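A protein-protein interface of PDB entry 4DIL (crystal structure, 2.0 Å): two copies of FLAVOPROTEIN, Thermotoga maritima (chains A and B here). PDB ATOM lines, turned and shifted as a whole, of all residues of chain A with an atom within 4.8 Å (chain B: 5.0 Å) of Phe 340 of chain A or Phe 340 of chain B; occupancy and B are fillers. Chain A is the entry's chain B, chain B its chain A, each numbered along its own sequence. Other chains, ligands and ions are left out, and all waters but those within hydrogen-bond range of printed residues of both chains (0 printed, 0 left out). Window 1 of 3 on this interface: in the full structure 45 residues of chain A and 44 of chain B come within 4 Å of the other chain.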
ATOM      1  N   VAL A  43     -26.485  13.896   8.825  1.00  0.00           N
ATOM      2  CA  VAL A  43     -25.750  14.708   7.860  1.00  0.00           C
ATOM      3  C   VAL A  43     -26.333  16.094   7.615  1.00  0.00           C
ATOM      4  O   VAL A  43     -25.585  17.045   7.451  1.00  0.00           O
ATOM      5  CB  VAL A  43     -25.521  13.965   6.511  1.00  0.00           C
ATOM      6  CG1 VAL A  43     -26.826  13.640   5.849  1.00  0.00           C
ATOM      7  CG2 VAL A  43     -24.638  14.788   5.576  1.00  0.00           C
ATOM      8  N   ILE A 310     -24.217  22.330   4.167  1.00  0.00           N
ATOM      9  CA  ILE A 310     -24.670  21.736   2.913  1.00  0.00           C
ATOM     10  C   ILE A 310     -26.206  21.760   2.781  1.00  0.00           C
ATOM     11  O   ILE A 310     -26.723  21.953   1.695  1.00  0.00           O
ATOM     12  CB  ILE A 310     -24.127  20.298   2.727  1.00  0.00           C
ATOM     13  CG1 ILE A 310     -24.477  19.766   1.334  1.00  0.00           C
ATOM     14  CG2 ILE A 310     -24.685  19.359   3.796  1.00  0.00           C
ATOM     15  CD1 ILE A 310     -23.771  20.498   0.217  1.00  0.00           C
ATOM     16  N   PRO A 336     -12.180  18.980  -1.915  1.00  0.00           N
ATOM     17  CA  PRO A 336     -13.032  17.975  -1.251  1.00  0.00           C
ATOM     18  C   PRO A 336     -14.447  18.454  -0.889  1.00  0.00           C
ATOM     19  O   PRO A 336     -15.431  17.711  -1.065  1.00  0.00           O
ATOM     20  CB  PRO A 336     -12.252  17.638   0.030  1.00  0.00           C
ATOM     21  CG  PRO A 336     -10.820  17.974  -0.292  1.00  0.00           C
ATOM     22  CD  PRO A 336     -10.884  19.144  -1.229  1.00  0.00           C
ATOM     23  N   LEU A 337     -14.542  19.672  -0.365  1.00  0.00           N
ATOM     24  CA  LEU A 337     -15.828  20.220   0.026  1.00  0.00           C
ATOM     25  C   LEU A 337     -16.666  20.587  -1.187  1.00  0.00           C
ATOM     26  O   LEU A 337     -17.876  20.480  -1.147  1.00  0.00           O
ATOM     27  CB  LEU A 337     -15.669  21.413   0.961  1.00  0.00           C
ATOM     28  CG  LEU A 337     -15.165  20.967   2.331  1.00  0.00           C
ATOM     29  CD1 LEU A 337     -14.998  22.161   3.236  1.00  0.00           C
ATOM     30  CD2 LEU A 337     -16.139  19.955   2.931  1.00  0.00           C
ATOM     31  N   MET A 338     -16.026  21.003  -2.266  1.00  0.00           N
ATOM     32  CA  MET A 338     -16.767  21.269  -3.487  1.00  0.00           C
ATOM     33  C   MET A 338     -17.174  19.969  -4.166  1.00  0.00           C
ATOM     34  O   MET A 338     -18.229  19.909  -4.785  1.00  0.00           O
ATOM     35  CB  MET A 338     -15.978  22.166  -4.447  1.00  0.00           C
ATOM     36  CG  MET A 338     -15.842  23.632  -3.985  1.00  0.00           C
ATOM     37  SD  MET A 338     -17.354  24.593  -4.290  1.00  0.00           S
ATOM     38  CE  MET A 338     -18.006  23.672  -5.695  1.00  0.00           C
ATOM     39  N   ARG A 339     -16.344  18.932  -4.049  1.00  0.00           N
ATOM     40  CA  ARG A 339     -16.721  17.625  -4.582  1.00  0.00           C
ATOM     41  C   ARG A 339     -17.968  17.129  -3.860  1.00  0.00           C
ATOM     42  O   ARG A 339     -18.940  16.703  -4.478  1.00  0.00           O
ATOM     43  CB  ARG A 339     -15.599  16.596  -4.418  1.00  0.00           C
ATOM     44  CG  ARG A 339     -16.014  15.200  -4.929  1.00  0.00           C
ATOM     45  CD  ARG A 339     -15.057  14.110  -4.457  1.00  0.00           C
ATOM     46  NE  ARG A 339     -15.121  13.905  -3.010  1.00  0.00           N
ATOM     47  CZ  ARG A 339     -14.092  14.027  -2.177  1.00  0.00           C
ATOM     48  NH1 ARG A 339     -12.889  14.358  -2.629  1.00  0.00           N
ATOM     49  NH2 ARG A 339     -14.268  13.813  -0.880  1.00  0.00           N
ATOM     50  N   PHE A 340     -17.927  17.200  -2.536  1.00  0.00           N
ATOM     51  CA  PHE A 340     -19.043  16.772  -1.714  1.00  0.00           C
ATOM     52  C   PHE A 340     -20.302  17.558  -2.080  1.00  0.00           C
ATOM     53  O   PHE A 340     -21.392  16.999  -2.222  1.00  0.00           O
ATOM     54  CB  PHE A 340     -18.692  16.973  -0.244  1.00  0.00           C
ATOM     55  CG  PHE A 340     -19.776  16.546   0.697  1.00  0.00           C
ATOM     56  CD1 PHE A 340     -19.866  15.227   1.122  1.00  0.00           C
ATOM     57  CD2 PHE A 340     -20.701  17.466   1.167  1.00  0.00           C
ATOM     58  CE1 PHE A 340     -20.877  14.824   1.987  1.00  0.00           C
ATOM     59  CE2 PHE A 340     -21.706  17.075   2.036  1.00  0.00           C
ATOM     60  CZ  PHE A 340     -21.796  15.748   2.447  1.00  0.00           C
ATOM     61  N   THR A 341     -20.149  18.866  -2.227  1.00  0.00           N
ATOM     62  CA  THR A 341     -21.297  19.710  -2.519  1.00  0.00           C
ATOM     63  C   THR A 341     -21.887  19.346  -3.876  1.00  0.00           C
ATOM     64  O   THR A 341     -23.084  19.138  -3.991  1.00  0.00           O
ATOM     65  CB  THR A 341     -20.911  21.189  -2.432  1.00  0.00           C
ATOM     66  OG1 THR A 341     -20.552  21.493  -1.073  1.00  0.00           O
ATOM     67  CG2 THR A 341     -22.062  22.082  -2.870  1.00  0.00           C
ATOM     68  N   LEU A 342     -21.038  19.222  -4.890  1.00  0.00           N
ATOM     69  CA  LEU A 342     -21.499  18.841  -6.226  1.00  0.00           C
ATOM     70  C   LEU A 342     -22.204  17.494  -6.240  1.00  0.00           C
ATOM     71  O   LEU A 342     -23.245  17.356  -6.876  1.00  0.00           O
ATOM     72  CB  LEU A 342     -20.344  18.833  -7.227  1.00  0.00           C
ATOM     73  CG  LEU A 342     -19.895  20.224  -7.685  1.00  0.00           C
ATOM     74  CD1 LEU A 342     -18.589  20.153  -8.464  1.00  0.00           C
ATOM     75  CD2 LEU A 342     -20.977  20.840  -8.538  1.00  0.00           C
ATOM     76  N   LEU A 343     -21.636  16.502  -5.549  1.00  0.00           N
ATOM     77  CA  LEU A 343     -22.247  15.172  -5.475  1.00  0.00           C
ATOM     78  C   LEU A 343     -23.604  15.199  -4.768  1.00  0.00           C
ATOM     79  O   LEU A 343     -24.518  14.471  -5.136  1.00  0.00           O
ATOM     80  CB  LEU A 343     -21.313  14.164  -4.789  1.00  0.00           C
ATOM     81  CG  LEU A 343     -20.080  13.614  -5.521  1.00  0.00           C
ATOM     82  CD1 LEU A 343     -19.270  12.722  -4.575  1.00  0.00           C
ATOM     83  CD2 LEU A 343     -20.478  12.825  -6.773  1.00  0.00           C
ATOM     84  N   GLU A 344     -23.752  16.034  -3.746  1.00  0.00           N
ATOM     85  CA  GLU A 344     -25.038  16.090  -3.058  1.00  0.00           C
ATOM     86  C   GLU A 344     -26.059  16.844  -3.907  1.00  0.00           C
ATOM     87  O   GLU A 344     -27.251  16.522  -3.913  1.00  0.00           O
ATOM     88  CB  GLU A 344     -24.903  16.717  -1.668  1.00  0.00           C
ATOM     89  CG  GLU A 344     -24.150  15.850  -0.667  1.00  0.00           C
ATOM     90  CD  GLU A 344     -24.594  14.398  -0.702  1.00  0.00           C
ATOM     91  OE1 GLU A 344     -25.813  14.122  -0.638  1.00  0.00           O
ATOM     92  OE2 GLU A 344     -23.722  13.516  -0.806  1.00  0.00           O
ATOM     93  N   VAL B  43     -10.421  23.362   4.211  1.00  0.00           N
ATOM     94  CA  VAL B  43     -11.086  22.111   4.578  1.00  0.00           C
ATOM     95  C   VAL B  43     -10.646  21.486   5.914  1.00  0.00           C
ATOM     96  O   VAL B  43     -11.494  21.089   6.710  1.00  0.00           O
ATOM     97  CB  VAL B  43     -11.037  21.059   3.442  1.00  0.00           C
ATOM     98  CG1 VAL B  43      -9.621  20.812   2.982  1.00  0.00           C
ATOM     99  CG2 VAL B  43     -11.674  19.761   3.900  1.00  0.00           C
ATOM    100  N   ILE B 310     -12.692  15.630   9.957  1.00  0.00           N
ATOM    101  CA  ILE B 310     -12.018  14.721   9.023  1.00  0.00           C
ATOM    102  C   ILE B 310     -10.492  14.783   9.192  1.00  0.00           C
ATOM    103  O   ILE B 310      -9.792  13.792   8.950  1.00  0.00           O
ATOM    104  CB  ILE B 310     -12.453  14.952   7.553  1.00  0.00           C
ATOM    105  CG1 ILE B 310     -11.771  13.966   6.612  1.00  0.00           C
ATOM    106  CG2 ILE B 310     -12.150  16.370   7.090  1.00  0.00           C
ATOM    107  CD1 ILE B 310     -12.164  12.542   6.842  1.00  0.00           C
ATOM    108  N   PRO B 336     -23.496   9.591   3.031  1.00  0.00           N
ATOM    109  CA  PRO B 336     -22.651  10.635   2.425  1.00  0.00           C
ATOM    110  C   PRO B 336     -21.374  10.941   3.193  1.00  0.00           C
ATOM    111  O   PRO B 336     -20.336  11.083   2.554  1.00  0.00           O
ATOM    112  CB  PRO B 336     -23.561  11.872   2.423  1.00  0.00           C
ATOM    113  CG  PRO B 336     -24.934  11.327   2.418  1.00  0.00           C
ATOM    114  CD  PRO B 336     -24.878  10.064   3.239  1.00  0.00           C
ATOM    115  N   LEU B 337     -21.437  11.030   4.518  1.00  0.00           N
ATOM    116  CA  LEU B 337     -20.249  11.364   5.308  1.00  0.00           C
ATOM    117  C   LEU B 337     -19.244  10.211   5.355  1.00  0.00           C
ATOM    118  O   LEU B 337     -18.041  10.434   5.512  1.00  0.00           O
ATOM    119  CB  LEU B 337     -20.626  11.830   6.715  1.00  0.00           C
ATOM    120  CG  LEU B 337     -21.561  13.038   6.751  1.00  0.00           C
ATOM    121  CD1 LEU B 337     -21.805  13.495   8.171  1.00  0.00           C
ATOM    122  CD2 LEU B 337     -20.984  14.171   5.937  1.00  0.00           C
ATOM    123  N   MET B 338     -19.737   8.983   5.214  1.00  0.00           N
ATOM    124  CA  MET B 338     -18.850   7.829   5.095  1.00  0.00           C
ATOM    125  C   MET B 338     -18.237   7.787   3.701  1.00  0.00           C
ATOM    126  O   MET B 338     -17.060   7.470   3.553  1.00  0.00           O
ATOM    127  CB  MET B 338     -19.572   6.519   5.443  1.00  0.00           C
ATOM    128  CG  MET B 338     -19.881   6.350   6.938  1.00  0.00           C
ATOM    129  SD  MET B 338     -18.387   6.408   7.981  1.00  0.00           S
ATOM    130  CE  MET B 338     -17.610   4.863   7.505  1.00  0.00           C
ATOM    131  N   ARG B 339     -19.020   8.131   2.677  1.00  0.00           N
ATOM    132  CA  ARG B 339     -18.448   8.241   1.328  1.00  0.00           C
ATOM    133  C   ARG B 339     -17.310   9.257   1.347  1.00  0.00           C
ATOM    134  O   ARG B 339     -16.200   8.982   0.888  1.00  0.00           O
ATOM    135  CB  ARG B 339     -19.495   8.669   0.289  1.00  0.00           C
ATOM    136  CG  ARG B 339     -18.946   8.674  -1.143  1.00  0.00           C
ATOM    137  CD  ARG B 339     -19.798   9.511  -2.099  1.00  0.00           C
ATOM    138  NE  ARG B 339     -19.802  10.932  -1.745  1.00  0.00           N
ATOM    139  CZ  ARG B 339     -20.896  11.636  -1.464  1.00  0.00           C
ATOM    140  NH1 ARG B 339     -22.091  11.064  -1.510  1.00  0.00           N
ATOM    141  NH2 ARG B 339     -20.796  12.926  -1.150  1.00  0.00           N
ATOM    142  N   PHE B 340     -17.597  10.425   1.909  1.00  0.00           N
ATOM    143  CA  PHE B 340     -16.620  11.493   2.006  1.00  0.00           C
ATOM    144  C   PHE B 340     -15.381  11.014   2.753  1.00  0.00           C
ATOM    145  O   PHE B 340     -14.253  11.210   2.298  1.00  0.00           O
ATOM    146  CB  PHE B 340     -17.229  12.711   2.696  1.00  0.00           C
ATOM    147  CG  PHE B 340     -16.272  13.854   2.850  1.00  0.00           C
ATOM    148  CD1 PHE B 340     -16.069  14.749   1.805  1.00  0.00           C
ATOM    149  CD2 PHE B 340     -15.572  14.036   4.035  1.00  0.00           C
ATOM    150  CE1 PHE B 340     -15.177  15.814   1.940  1.00  0.00           C
ATOM    151  CE2 PHE B 340     -14.675  15.093   4.185  1.00  0.00           C
ATOM    152  CZ  PHE B 340     -14.474  15.983   3.141  1.00  0.00           C
ATOM    153  N   THR B 341     -15.588  10.370   3.895  1.00  0.00           N
ATOM    154  CA  THR B 341     -14.454   9.950   4.707  1.00  0.00           C
ATOM    155  C   THR B 341     -13.584   8.929   3.990  1.00  0.00           C
ATOM    156  O   THR B 341     -12.351   9.053   3.990  1.00  0.00           O
ATOM    157  CB  THR B 341     -14.891   9.438   6.077  1.00  0.00           C
ATOM    158  OG1 THR B 341     -15.594  10.481   6.758  1.00  0.00           O
ATOM    159  CG2 THR B 341     -13.670   9.030   6.914  1.00  0.00           C
ATOM    160  N   LEU B 342     -14.218   7.936   3.369  1.00  0.00           N
ATOM    161  CA  LEU B 342     -13.487   6.903   2.634  1.00  0.00           C
ATOM    162  C   LEU B 342     -12.696   7.516   1.494  1.00  0.00           C
ATOM    163  O   LEU B 342     -11.535   7.164   1.271  1.00  0.00           O
ATOM    164  CB  LEU B 342     -14.437   5.829   2.095  1.00  0.00           C
ATOM    165  CG  LEU B 342     -15.003   4.823   3.099  1.00  0.00           C
ATOM    166  CD1 LEU B 342     -16.120   3.997   2.442  1.00  0.00           C
ATOM    167  CD2 LEU B 342     -13.920   3.916   3.651  1.00  0.00           C
ATOM    168  N   LEU B 343     -13.314   8.450   0.780  1.00  0.00           N
ATOM    169  CA  LEU B 343     -12.639   9.110  -0.329  1.00  0.00           C
ATOM    170  C   LEU B 343     -11.401   9.884   0.139  1.00  0.00           C
ATOM    171  O   LEU B 343     -10.365   9.859  -0.519  1.00  0.00           O
ATOM    172  CB  LEU B 343     -13.607  10.021  -1.091  1.00  0.00           C
ATOM    173  CG  LEU B 343     -14.608   9.347  -2.034  1.00  0.00           C
ATOM    174  CD1 LEU B 343     -15.500  10.390  -2.686  1.00  0.00           C
ATOM    175  CD2 LEU B 343     -13.912   8.504  -3.101  1.00  0.00           C
ATOM    176  N   GLU B 344     -11.496  10.570   1.272  1.00  0.00           N
ATOM    177  CA  GLU B 344     -10.321  11.288   1.801  1.00  0.00           C
ATOM    178  C   GLU B 344      -9.231  10.338   2.308  1.00  0.00           C
ATOM    179  O   GLU B 344      -8.039  10.584   2.112  1.00  0.00           O
ATOM    180  CB  GLU B 344     -10.723  12.285   2.894  1.00  0.00           C
ATOM    181  CG  GLU B 344     -11.553  13.437   2.365  1.00  0.00           C
ATOM    182  CD  GLU B 344     -10.935  14.064   1.129  1.00  0.00           C
ATOM    183  OE1 GLU B 344      -9.742  14.447   1.185  1.00  0.00           O
ATOM    184  OE2 GLU B 344     -11.627  14.162   0.095  1.00  0.00           O
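The guanidinium group of Arg 339 of chain B lies within salt-bridge range of the side-chain carboxylate of Glu 344 of chain A (3.0 Å). NH2 of Arg 339 of chain A is in salt-bridge range of OE2 of Glu 344 of chain B (2.8 Å).
The side-chain hydroxyl of Thr 341 of chain B sits at hydrogen-bond distance from the backbone carbonyl oxygen of Leu 337 of chain B.
Among the printed residues, merely in contact across the chains: Phe 340 of chain A with Arg 339 of chain B (3.4 Å), Arg 339 of chain A with Phe 340 of chain B (3.4 Å), Leu 343 of chain A with Arg 339 of chain B (3.4 Å), Pro 336 of chain A with Glu 344 of chain B (3.5 Å), Arg 339 of chain A with Leu 343 of chain B (3.6 Å), Pro 336 of chain A with Phe 340 of chain B (3.6 Å), Glu 344 of chain A with Pro 336 of chain B (3.6 Å), Val 43 of chain A with Leu 337 of chain B (3.7 Å), Phe 340 of chain A with Pro 336 of chain B (3.8 Å), Phe 340 of chain A with Phe 340 of chain B (3.9 Å) and Phe 340 of chain A with Leu 337 of chain B (3.9 Å).
Leu 337 of chain A touches none of the printed residues of chain B. Met 338 of chain A touches none of the printed residues of chain B. Phe 340 of chain A touches four residues of chain B. Of the printed residues of chain B, Leu 343 of chain A touches Arg 339 (3.4 Å). Printed residues of chain B within 4 Å of Glu 344 of chain A: Pro 336 and Arg 339. Of the printed residues of chain A, Pro 336 of chain B touches Phe 340 and Glu 344. Printed residues of chain A within 4 Å of Arg 339 of chain B: Phe 340, Leu 343 and Glu 344. Of the printed residues of chain A, Leu 343 of chain B touches Arg 339. The nearest printed residue of chain B that does not touch Phe 340 of chain A is Met 338 of chain B (6.8 Å). The nearest residue of chain A that does not touch Phe 340 of chain B is Leu 337 of chain A (4.3 Å).
Of the 11 printed residues of chain A, 6 touch a printed residue of chain B. Hydrophobic or aromatic side chains of chain B that line the printed part of chain A: Pro 336, Leu 337, Phe 340 and Leu 343. Among the printed residues, 13 pairs touch across the chains. Among the printed residues, Asp or Glu carboxylates within 4 Å of a Lys or Arg side-chain nitrogen of the other chain: Arg 339 of chain A with Glu 344 of chain B (2.8 Å) and Glu 344 of chain A with Arg 339 of chain B (3.0 Å).
Val 43 of chain A touches Leu 337 of chain B, but with the chains exchanged Leu 337 of chain A does not touch Val 43 of chain B (4.01 Å). Arg 339 of chain A touches Leu 343 of chain B, and with the chains exchanged Leu 343 of chain A touches Arg 339 of chain B. Arg 339 of chain A touches Glu 344 of chain B, and with the chains exchanged Glu 344 of chain A touches Arg 339 of chain B. Phe 340 of chain A touches Leu 337 of chain B, but with the chains exchanged Leu 337 of chain A does not touch Phe 340 of chain B (4.3 Å). Positions printed for both chains: 43, 310, 336, 337, 338, 339, 340, 341, 342, 343 and 344. Of the 13 pairs that touch across the chains among the printed residues, 11 have their exchanged pair printed and touching as well.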
